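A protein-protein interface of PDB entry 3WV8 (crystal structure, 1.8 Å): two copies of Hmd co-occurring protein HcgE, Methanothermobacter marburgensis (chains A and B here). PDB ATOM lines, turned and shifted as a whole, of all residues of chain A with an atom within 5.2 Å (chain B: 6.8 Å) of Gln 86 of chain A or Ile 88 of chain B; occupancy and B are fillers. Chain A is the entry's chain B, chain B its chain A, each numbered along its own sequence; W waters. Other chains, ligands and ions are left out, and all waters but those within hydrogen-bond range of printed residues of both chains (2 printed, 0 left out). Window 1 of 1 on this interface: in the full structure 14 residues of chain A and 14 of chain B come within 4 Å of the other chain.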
ATOM      1  N   ILE A  43      18.084 -13.639  -4.995  1.00  0.00           N
ATOM      2  CA  ILE A  43      18.524 -14.175  -6.285  1.00  0.00           C
ATOM      3  C   ILE A  43      18.374 -15.630  -6.264  1.00  0.00           C
ATOM      4  O   ILE A  43      19.011 -16.335  -5.430  1.00  0.00           O
ATOM      5  CB  ILE A  43      19.994 -13.746  -6.552  1.00  0.00           C
ATOM      6  CG1 ILE A  43      20.012 -12.192  -6.578  1.00  0.00           C
ATOM      7  CG2 ILE A  43      20.489 -14.381  -7.886  1.00  0.00           C
ATOM      8  CD1 ILE A  43      21.404 -11.581  -6.486  1.00  0.00           C
ATOM      9  N   LYS A  44      17.613 -16.147  -7.240  1.00  0.00           N
ATOM     10  CA  LYS A  44      17.286 -17.547  -7.312  1.00  0.00           C
ATOM     11  C   LYS A  44      17.999 -18.071  -8.596  1.00  0.00           C
ATOM     12  O   LYS A  44      17.709 -17.597  -9.717  1.00  0.00           O
ATOM     13  CB  LYS A  44      15.773 -17.614  -7.468  1.00  0.00           C
ATOM     14  CG  LYS A  44      15.399 -19.086  -7.554  1.00  0.00           C
ATOM     15  CD  LYS A  44      13.887 -19.278  -7.493  1.00  0.00           C
ATOM     16  CE  LYS A  44      13.156 -18.828  -6.264  1.00  0.00           C
ATOM     17  NZ  LYS A  44      11.872 -19.548  -6.258  1.00  0.00           N
ATOM     18  N   VAL A  45      18.878 -19.023  -8.457  1.00  0.00           N
ATOM     19  CA  VAL A  45      19.640 -19.498  -9.567  1.00  0.00           C
ATOM     20  C   VAL A  45      19.275 -20.944  -9.874  1.00  0.00           C
ATOM     21  O   VAL A  45      19.296 -21.825  -8.993  1.00  0.00           O
ATOM     22  CB  VAL A  45      21.155 -19.428  -9.286  1.00  0.00           C
ATOM     23  CG1 VAL A  45      21.766 -19.620 -10.616  1.00  0.00           C
ATOM     24  CG2 VAL A  45      21.390 -17.967  -8.956  1.00  0.00           C
ATOM     25  N   GLU A  74      25.555 -20.359  -4.583  1.00  0.00           N
ATOM     26  CA  GLU A  74      24.917 -20.122  -3.309  1.00  0.00           C
ATOM     27  C   GLU A  74      26.005 -20.116  -2.248  1.00  0.00           C
ATOM     28  O   GLU A  74      25.859 -19.320  -1.281  1.00  0.00           O
ATOM     29  CB  GLU A  74      23.792 -21.217  -3.076  1.00  0.00           C
ATOM     30  CG  GLU A  74      23.211 -21.135  -1.679  1.00  0.00           C
ATOM     31  CD  GLU A  74      21.920 -21.950  -1.414  1.00  0.00           C
ATOM     32  OE1 GLU A  74      21.258 -22.617  -2.324  1.00  0.00           O
ATOM     33  OE2 GLU A  74      21.521 -21.797  -0.239  1.00  0.00           O
ATOM     34  N   THR A  84      19.797 -12.695  -0.184  1.00  0.00           N
ATOM     35  CA  THR A  84      19.558 -14.090  -0.121  1.00  0.00           C
ATOM     36  C   THR A  84      19.775 -14.667  -1.505  1.00  0.00           C
ATOM     37  O   THR A  84      19.245 -14.074  -2.456  1.00  0.00           O
ATOM     38  CB  THR A  84      18.139 -14.340   0.451  1.00  0.00           C
ATOM     39  OG1 THR A  84      18.107 -13.950   1.844  1.00  0.00           O
ATOM     40  CG2 THR A  84      17.741 -15.795   0.394  1.00  0.00           C
ATOM     41  N   VAL A  85      20.597 -15.731  -1.610  1.00  0.00           N
ATOM     42  CA  VAL A  85      20.884 -16.427  -2.935  1.00  0.00           C
ATOM     43  C   VAL A  85      20.466 -17.888  -2.745  1.00  0.00           C
ATOM     44  O   VAL A  85      20.870 -18.514  -1.760  1.00  0.00           O
ATOM     45  CB  VAL A  85      22.354 -16.317  -3.222  1.00  0.00           C
ATOM     46  CG1 VAL A  85      22.830 -17.153  -4.446  1.00  0.00           C
ATOM     47  CG2 VAL A  85      22.748 -14.825  -3.403  1.00  0.00           C
ATOM     48  N   GLN A  86      19.675 -18.412  -3.654  1.00  0.00           N
ATOM     49  CA  GLN A  86      19.126 -19.762  -3.636  1.00  0.00           C
ATOM     50  C   GLN A  86      19.405 -20.452  -4.902  1.00  0.00           C
ATOM     51  O   GLN A  86      19.069 -19.961  -5.987  1.00  0.00           O
ATOM     52  CB  GLN A  86      17.601 -19.762  -3.445  1.00  0.00           C
ATOM     53  CG  GLN A  86      17.034 -21.152  -3.371  1.00  0.00           C
ATOM     54  CD  GLN A  86      15.531 -21.099  -3.320  1.00  0.00           C
ATOM     55  OE1 GLN A  86      14.917 -20.039  -3.004  1.00  0.00           O
ATOM     56  NE2 GLN A  86      14.920 -22.274  -3.525  1.00  0.00           N
ATOM     57  N   GLY A  87      20.060 -21.587  -4.758  1.00  0.00           N
ATOM     58  CA  GLY A  87      20.528 -22.422  -5.882  1.00  0.00           C
ATOM     59  C   GLY A  87      19.617 -23.624  -5.884  1.00  0.00           C
ATOM     60  O   GLY A  87      19.488 -24.318  -4.796  1.00  0.00           O
ATOM     61  N   ILE A  88      18.974 -23.861  -7.019  1.00  0.00           N
ATOM     62  CA  ILE A  88      18.159 -25.089  -7.281  1.00  0.00           C
ATOM     63  C   ILE A  88      18.748 -25.838  -8.448  1.00  0.00           C
ATOM     64  O   ILE A  88      18.764 -25.323  -9.686  1.00  0.00           O
ATOM     65  CB  ILE A  88      16.699 -24.699  -7.678  1.00  0.00           C
ATOM     66  CG1 ILE A  88      16.104 -23.821  -6.531  1.00  0.00           C
ATOM     67  CG2 ILE A  88      15.899 -25.960  -8.028  1.00  0.00           C
ATOM     68  CD1 ILE A  88      14.753 -23.083  -6.848  1.00  0.00           C
ATOM     69  N   LEU A  99       8.787 -23.678 -10.319  1.00  0.00           N
ATOM     70  CA  LEU A  99      10.011 -23.022  -9.816  1.00  0.00           C
ATOM     71  C   LEU A  99      10.123 -21.623 -10.425  1.00  0.00           C
ATOM     72  O   LEU A  99      10.850 -20.782  -9.990  1.00  0.00           O
ATOM     73  CB  LEU A  99      11.248 -23.916 -10.134  1.00  0.00           C
ATOM     74  CG  LEU A  99      11.265 -25.492  -9.864  1.00  0.00           C
ATOM     75  CD1 LEU A  99      12.502 -26.136 -10.532  1.00  0.00           C
ATOM     76  CD2 LEU A  99      11.119 -26.020  -8.411  1.00  0.00           C
ATOM     77  N   LYS B  44      15.650 -25.103   4.820  1.00  0.00           N
ATOM     78  CA  LYS B  44      15.214 -25.380   3.436  1.00  0.00           C
ATOM     79  C   LYS B  44      13.953 -26.229   3.710  1.00  0.00           C
ATOM     80  O   LYS B  44      14.001 -27.189   4.498  1.00  0.00           O
ATOM     81  CB  LYS B  44      16.334 -26.113   2.647  1.00  0.00           C
ATOM     82  CG  LYS B  44      15.902 -26.645   1.301  1.00  0.00           C
ATOM     83  CD  LYS B  44      17.042 -27.233   0.403  1.00  0.00           C
ATOM     84  CE  LYS B  44      18.260 -26.387   0.029  1.00  0.00           C
ATOM     85  NZ  LYS B  44      19.033 -27.219  -0.970  1.00  0.00           N
ATOM     86  N   VAL B  45      12.870 -25.944   3.031  1.00  0.00           N
ATOM     87  CA  VAL B  45      11.633 -26.704   3.220  1.00  0.00           C
ATOM     88  C   VAL B  45      11.181 -27.250   1.891  1.00  0.00           C
ATOM     89  O   VAL B  45      11.074 -26.487   0.960  1.00  0.00           O
ATOM     90  CB  VAL B  45      10.483 -25.804   3.711  1.00  0.00           C
ATOM     91  CG1 VAL B  45       9.408 -26.741   4.204  1.00  0.00           C
ATOM     92  CG2 VAL B  45      10.946 -24.892   4.799  1.00  0.00           C
ATOM     93  N   ILE B  46      10.945 -28.544   1.822  1.00  0.00           N
ATOM     94  CA  ILE B  46      10.635 -29.173   0.494  1.00  0.00           C
ATOM     95  C   ILE B  46       9.326 -29.967   0.546  1.00  0.00           C
ATOM     96  O   ILE B  46       9.191 -30.918   1.301  1.00  0.00           O
ATOM     97  CB  ILE B  46      11.831 -30.088   0.132  1.00  0.00           C
ATOM     98  CG1 ILE B  46      13.236 -29.373   0.292  1.00  0.00           C
ATOM     99  CG2 ILE B  46      11.664 -30.805  -1.237  1.00  0.00           C
ATOM    100  CD1 ILE B  46      14.459 -30.161  -0.165  1.00  0.00           C
ATOM    101  N   ASP B  47       8.329 -29.563  -0.267  1.00  0.00           N
ATOM    102  CA  ASP B  47       7.022 -30.255  -0.309  1.00  0.00           C
ATOM    103  C   ASP B  47       6.326 -29.840  -1.614  1.00  0.00           C
ATOM    104  O   ASP B  47       6.472 -28.677  -2.039  1.00  0.00           O
ATOM    105  CB  ASP B  47       6.264 -29.717   0.875  1.00  0.00           C
ATOM    106  CG  ASP B  47       4.992 -30.555   1.155  1.00  0.00           C
ATOM    107  OD1 ASP B  47       4.217 -30.903   0.205  1.00  0.00           O
ATOM    108  OD2 ASP B  47       4.757 -30.894   2.331  1.00  0.00           O
ATOM    109  N   GLY B  48       5.635 -30.762  -2.290  1.00  0.00           N
ATOM    110  CA  GLY B  48       5.095 -30.563  -3.621  1.00  0.00           C
ATOM    111  C   GLY B  48       3.661 -30.108  -3.540  1.00  0.00           C
ATOM    112  O   GLY B  48       3.018 -29.892  -4.593  1.00  0.00           O
ATOM    113  N   VAL B  70       5.311 -24.511   0.804  1.00  0.00           N
ATOM    114  CA  VAL B  70       6.605 -24.027   1.044  1.00  0.00           C
ATOM    115  C   VAL B  70       6.719 -22.517   0.785  1.00  0.00           C
ATOM    116  O   VAL B  70       7.661 -21.882   1.302  1.00  0.00           O
ATOM    117  CB  VAL B  70       7.701 -24.844   0.237  1.00  0.00           C
ATOM    118  CG1 VAL B  70       7.693 -26.301   0.714  1.00  0.00           C
ATOM    119  CG2 VAL B  70       7.390 -24.838  -1.279  1.00  0.00           C
ATOM    120  N   LYS B  71       5.941 -22.042  -0.173  1.00  0.00           N
ATOM    121  CA  LYS B  71       5.976 -20.641  -0.561  1.00  0.00           C
ATOM    122  C   LYS B  71       5.293 -19.806   0.509  1.00  0.00           C
ATOM    123  O   LYS B  71       5.792 -18.730   0.901  1.00  0.00           O
ATOM    124  CB  LYS B  71       5.137 -20.382  -1.809  1.00  0.00           C
ATOM    125  CG  LYS B  71       4.761 -18.887  -2.022  1.00  0.00           C
ATOM    126  CD  LYS B  71       5.901 -18.058  -2.591  1.00  0.00           C
ATOM    127  CE  LYS B  71       6.134 -16.765  -1.866  1.00  0.00           C
ATOM    128  NZ  LYS B  71       7.453 -17.102  -1.213  1.00  0.00           N
ATOM    129  N   GLU B  74       8.092 -19.676   3.221  1.00  0.00           N
ATOM    130  CA  GLU B  74       9.106 -18.727   2.753  1.00  0.00           C
ATOM    131  C   GLU B  74       8.655 -17.316   2.912  1.00  0.00           C
ATOM    132  O   GLU B  74       9.462 -16.416   3.191  1.00  0.00           O
ATOM    133  CB  GLU B  74       9.486 -19.016   1.249  1.00  0.00           C
ATOM    134  CG  GLU B  74      10.768 -18.197   0.998  1.00  0.00           C
ATOM    135  CD  GLU B  74      11.447 -18.487  -0.345  1.00  0.00           C
ATOM    136  OE1 GLU B  74      11.450 -19.671  -0.796  1.00  0.00           O
ATOM    137  OE2 GLU B  74      11.984 -17.448  -0.907  1.00  0.00           O
ATOM    138  N   THR B  84      17.876 -17.595   6.746  1.00  0.00           N
ATOM    139  CA  THR B  84      17.476 -17.776   5.381  1.00  0.00           C
ATOM    140  C   THR B  84      16.374 -18.892   5.380  1.00  0.00           C
ATOM    141  O   THR B  84      16.642 -19.961   5.864  1.00  0.00           O
ATOM    142  CB  THR B  84      18.697 -18.257   4.492  1.00  0.00           C
ATOM    143  OG1 THR B  84      19.662 -17.212   4.434  1.00  0.00           O
ATOM    144  CG2 THR B  84      18.226 -18.700   3.116  1.00  0.00           C
ATOM    145  N   VAL B  85      15.226 -18.664   4.749  1.00  0.00           N
ATOM    146  CA  VAL B  85      14.213 -19.735   4.589  1.00  0.00           C
ATOM    147  C   VAL B  85      14.021 -19.812   3.057  1.00  0.00           C
ATOM    148  O   VAL B  85      13.969 -18.783   2.378  1.00  0.00           O
ATOM    149  CB  VAL B  85      12.910 -19.437   5.361  1.00  0.00           C
ATOM    150  CG1 VAL B  85      11.917 -20.570   5.170  1.00  0.00           C
ATOM    151  CG2 VAL B  85      13.232 -19.197   6.846  1.00  0.00           C
ATOM    152  N   GLN B  86      14.150 -21.027   2.547  1.00  0.00           N
ATOM    153  CA  GLN B  86      14.117 -21.343   1.131  1.00  0.00           C
ATOM    154  C   GLN B  86      13.029 -22.396   0.974  1.00  0.00           C
ATOM    155  O   GLN B  86      13.095 -23.439   1.600  1.00  0.00           O
ATOM    156  CB  GLN B  86      15.472 -21.914   0.696  1.00  0.00           C
ATOM    157  CG  GLN B  86      16.676 -21.011   0.807  1.00  0.00           C
ATOM    158  CD  GLN B  86      18.030 -21.721   0.550  1.00  0.00           C
ATOM    159  OE1 GLN B  86      18.179 -22.951   0.644  1.00  0.00           O
ATOM    160  NE2 GLN B  86      19.004 -20.938   0.290  1.00  0.00           N
ATOM    161  N   GLY B  87      12.043 -22.200   0.098  1.00  0.00           N
ATOM    162  CA  GLY B  87      11.107 -23.276  -0.090  1.00  0.00           C
ATOM    163  C   GLY B  87      11.257 -23.824  -1.489  1.00  0.00           C
ATOM    164  O   GLY B  87      11.495 -23.025  -2.417  1.00  0.00           O
ATOM    165  N   ILE B  88      11.266 -25.137  -1.663  1.00  0.00           N
ATOM    166  CA  ILE B  88      11.300 -25.742  -3.033  1.00  0.00           C
ATOM    167  C   ILE B  88      10.007 -26.591  -3.120  1.00  0.00           C
ATOM    168  O   ILE B  88       9.739 -27.543  -2.225  1.00  0.00           O
ATOM    169  CB  ILE B  88      12.543 -26.686  -3.230  1.00  0.00           C
ATOM    170  CG1 ILE B  88      13.799 -25.990  -2.719  1.00  0.00           C
ATOM    171  CG2 ILE B  88      12.614 -27.188  -4.702  1.00  0.00           C
ATOM    172  CD1 ILE B  88      15.088 -26.820  -2.549  1.00  0.00           C
ATOM    173  N   PRO B  89       9.138 -26.226  -4.105  1.00  0.00           N
ATOM    174  CA  PRO B  89       7.811 -26.816  -4.234  1.00  0.00           C
ATOM    175  C   PRO B  89       7.753 -28.096  -5.013  1.00  0.00           C
ATOM    176  O   PRO B  89       6.899 -28.243  -5.951  1.00  0.00           O
ATOM    177  CB  PRO B  89       7.026 -25.725  -4.817  1.00  0.00           C
ATOM    178  CG  PRO B  89       8.026 -24.901  -5.675  1.00  0.00           C
ATOM    179  CD  PRO B  89       9.328 -25.055  -4.992  1.00  0.00           C
ATOM    180  N   GLU B  90       8.567 -29.080  -4.506  1.00  0.00           N
ATOM    181  CA  GLU B  90       8.577 -30.338  -5.233  1.00  0.00           C
ATOM    182  C   GLU B  90       8.502 -31.453  -4.280  1.00  0.00           C
ATOM    183  O   GLU B  90       9.007 -31.287  -3.145  1.00  0.00           O
ATOM    184  CB  GLU B  90       9.818 -30.503  -6.077  1.00  0.00           C
ATOM    185  CG  GLU B  90       9.967 -29.374  -7.143  1.00  0.00           C
ATOM    186  CD  GLU B  90      11.253 -29.561  -7.965  1.00  0.00           C
ATOM    187  OE1 GLU B  90      12.166 -30.249  -7.483  1.00  0.00           O
ATOM    188  OE2 GLU B  90      11.396 -29.051  -9.090  1.00  0.00           O
ATOM    189  N   TYR B  91       7.921 -32.574  -4.719  1.00  0.00           N
ATOM    190  CA  TYR B  91       8.125 -33.832  -3.943  1.00  0.00           C
ATOM    191  C   TYR B  91       9.601 -34.364  -4.050  1.00  0.00           C
ATOM    192  O   TYR B  91      10.233 -34.251  -5.119  1.00  0.00           O
ATOM    193  CB  TYR B  91       7.113 -34.901  -4.343  1.00  0.00           C
ATOM    194  CG  TYR B  91       5.688 -34.545  -4.084  1.00  0.00           C
ATOM    195  CD1 TYR B  91       5.192 -34.373  -2.787  1.00  0.00           C
ATOM    196  CD2 TYR B  91       4.854 -34.152  -5.161  1.00  0.00           C
ATOM    197  CE1 TYR B  91       3.879 -34.012  -2.579  1.00  0.00           C
ATOM    198  CE2 TYR B  91       3.543 -33.771  -5.001  1.00  0.00           C
ATOM    199  CZ  TYR B  91       3.028 -33.678  -3.739  1.00  0.00           C
ATOM    200  OH  TYR B  91       1.762 -33.161  -3.830  1.00  0.00           O
ATOM    201  N   LEU B  99      18.569 -32.367  -4.077  1.00  0.00           N
ATOM    202  CA  LEU B  99      17.914 -31.305  -3.328  1.00  0.00           C
ATOM    203  C   LEU B  99      18.239 -31.443  -1.841  1.00  0.00           C
ATOM    204  O   LEU B  99      18.274 -30.439  -1.163  1.00  0.00           O
ATOM    205  CB  LEU B  99      16.420 -31.337  -3.561  1.00  0.00           C
ATOM    206  CG  LEU B  99      15.899 -31.032  -4.978  1.00  0.00           C
ATOM    207  CD1 LEU B  99      14.374 -30.860  -5.017  1.00  0.00           C
ATOM    208  CD2 LEU B  99      16.556 -29.761  -5.554  1.00  0.00           C
HETATM  209  O   HOH W   1      18.409 -26.699  -3.639  1.00  0.00           O
HETATM  210  O   HOH W   2      12.154 -22.956  -5.026  1.00  0.00           O
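Printed residues of chain B within 4 Å of Gln 86 of chain A: Gly 87 and Ile 88. Printed residues of chain A within 4 Å of Ile 88 of chain B: Gln 86 (3.96 Å). Of the printed residues of chain A, Glu 90 of chain B touches Leu 99. Of the printed residues of chain A, Gly 87 of chain B touches Gln 86 (3.7 Å). Printed residues of chain B within 4 Å of Leu 99 of chain A: Pro 89 (3.98 Å) and Glu 90 (3.1 Å). Of the printed residues of chain A, Pro 89 of chain B touches Leu 99. Ile 46 of chain B touches none of the printed residues of chain A. Val 45 of chain B touches none of the printed residues of chain A. The nearest printed residue of chain B that does not touch Gln 86 of chain A is Gln 86 of chain B (4.1 Å). The nearest printed residue of chain A that does not touch Gln 86 of chain B is Gln 86 of chain A (4.1 Å).
Glu 74 of chain A touches Gln 86 of chain B, but with the chains exchanged Gln 86 of chain A does not touch Glu 74 of chain B (4.1 Å). Val 85 of chain A touches Gln 86 of chain B, but with the chains exchanged Gln 86 of chain A does not touch Val 85 of chain B (5.6 Å). Gln 86 of chain A touches Gly 87 of chain B, but with the chains exchanged Gly 87 of chain A does not touch Gln 86 of chain B (5.2 Å). Gln 86 of chain A touches Ile 88 of chain B, but with the chains exchanged Ile 88 of chain A does not touch Gln 86 of chain B (7.5 Å). Positions printed for both chains: 44, 45, 74, 84, 85, 86, 87, 88 and 99. Of the 6 pairs that touch across the chains among the printed residues, none has its exchanged pair printed and touching as well.
The side-chain amide nitrogen (NE2) of Gln 86 of chain B lies within hydrogen-bond range of the side-chain carboxylate (OE2) of Glu 74 of chain A, at 2.7 Å.
Among the printed residues, 6 pairs touch across the chains. Among the printed residues, no Asp or Glu carboxylate lies within 4 Å of a Lys or Arg side-chain nitrogen of the other chain.
Among the printed residues, pairs that only touch across the chains: Leu 99 of chain A with Glu 90 of chain B, Gln 86 of chain A with Gly 87 of chain B, Val 85 of chain A with Gln 86 of chain B, Gln 86 of chain A with Ile 88 of chain B and Leu 99 of chain A with Pro 89 of chain B.
Water W2 lies within hydrogen-bond range of the backbone carbonyl oxygen of Gly 87 of chain B (2.7 Å) and the side-chain amide nitrogen of Gln 86 of chain A (3.2 Å). Water W1 lies within hydrogen-bond range of the side-chain amino group (NZ) of Lys 44 of chain B and the backbone carbonyl oxygen (O) of Gly 87 of chain A.
The backbone NH (N) of Val 45 of chain B sits at hydrogen-bond distance from the backbone carbonyl oxygen (O) of Gln 86 of chain B (2.9 Å). O of Val 45 of chain B sits at hydrogen-bond distance from N of Ile 88 of chain B, at 3.0 Å. The backbone NH (N) of Asp 47 of chain B sits at hydrogen-bond distance from the backbone carbonyl oxygen (O) of Ile 88 of chain B (3.1 Å). The backbone carbonyl oxygen of Asp 47 of chain B sits at hydrogen-bond distance from the backbone NH of Glu 90 of chain B. The backbone carbonyl oxygen of Gln 86 of chain A lies within hydrogen-bond range of the backbone NH of Val 45 of chain A, at 2.6 Å. N of Gly 87 of chain A lies within hydrogen-bond range of OE1 of Glu 74 of chain A, at 2.9 Å.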
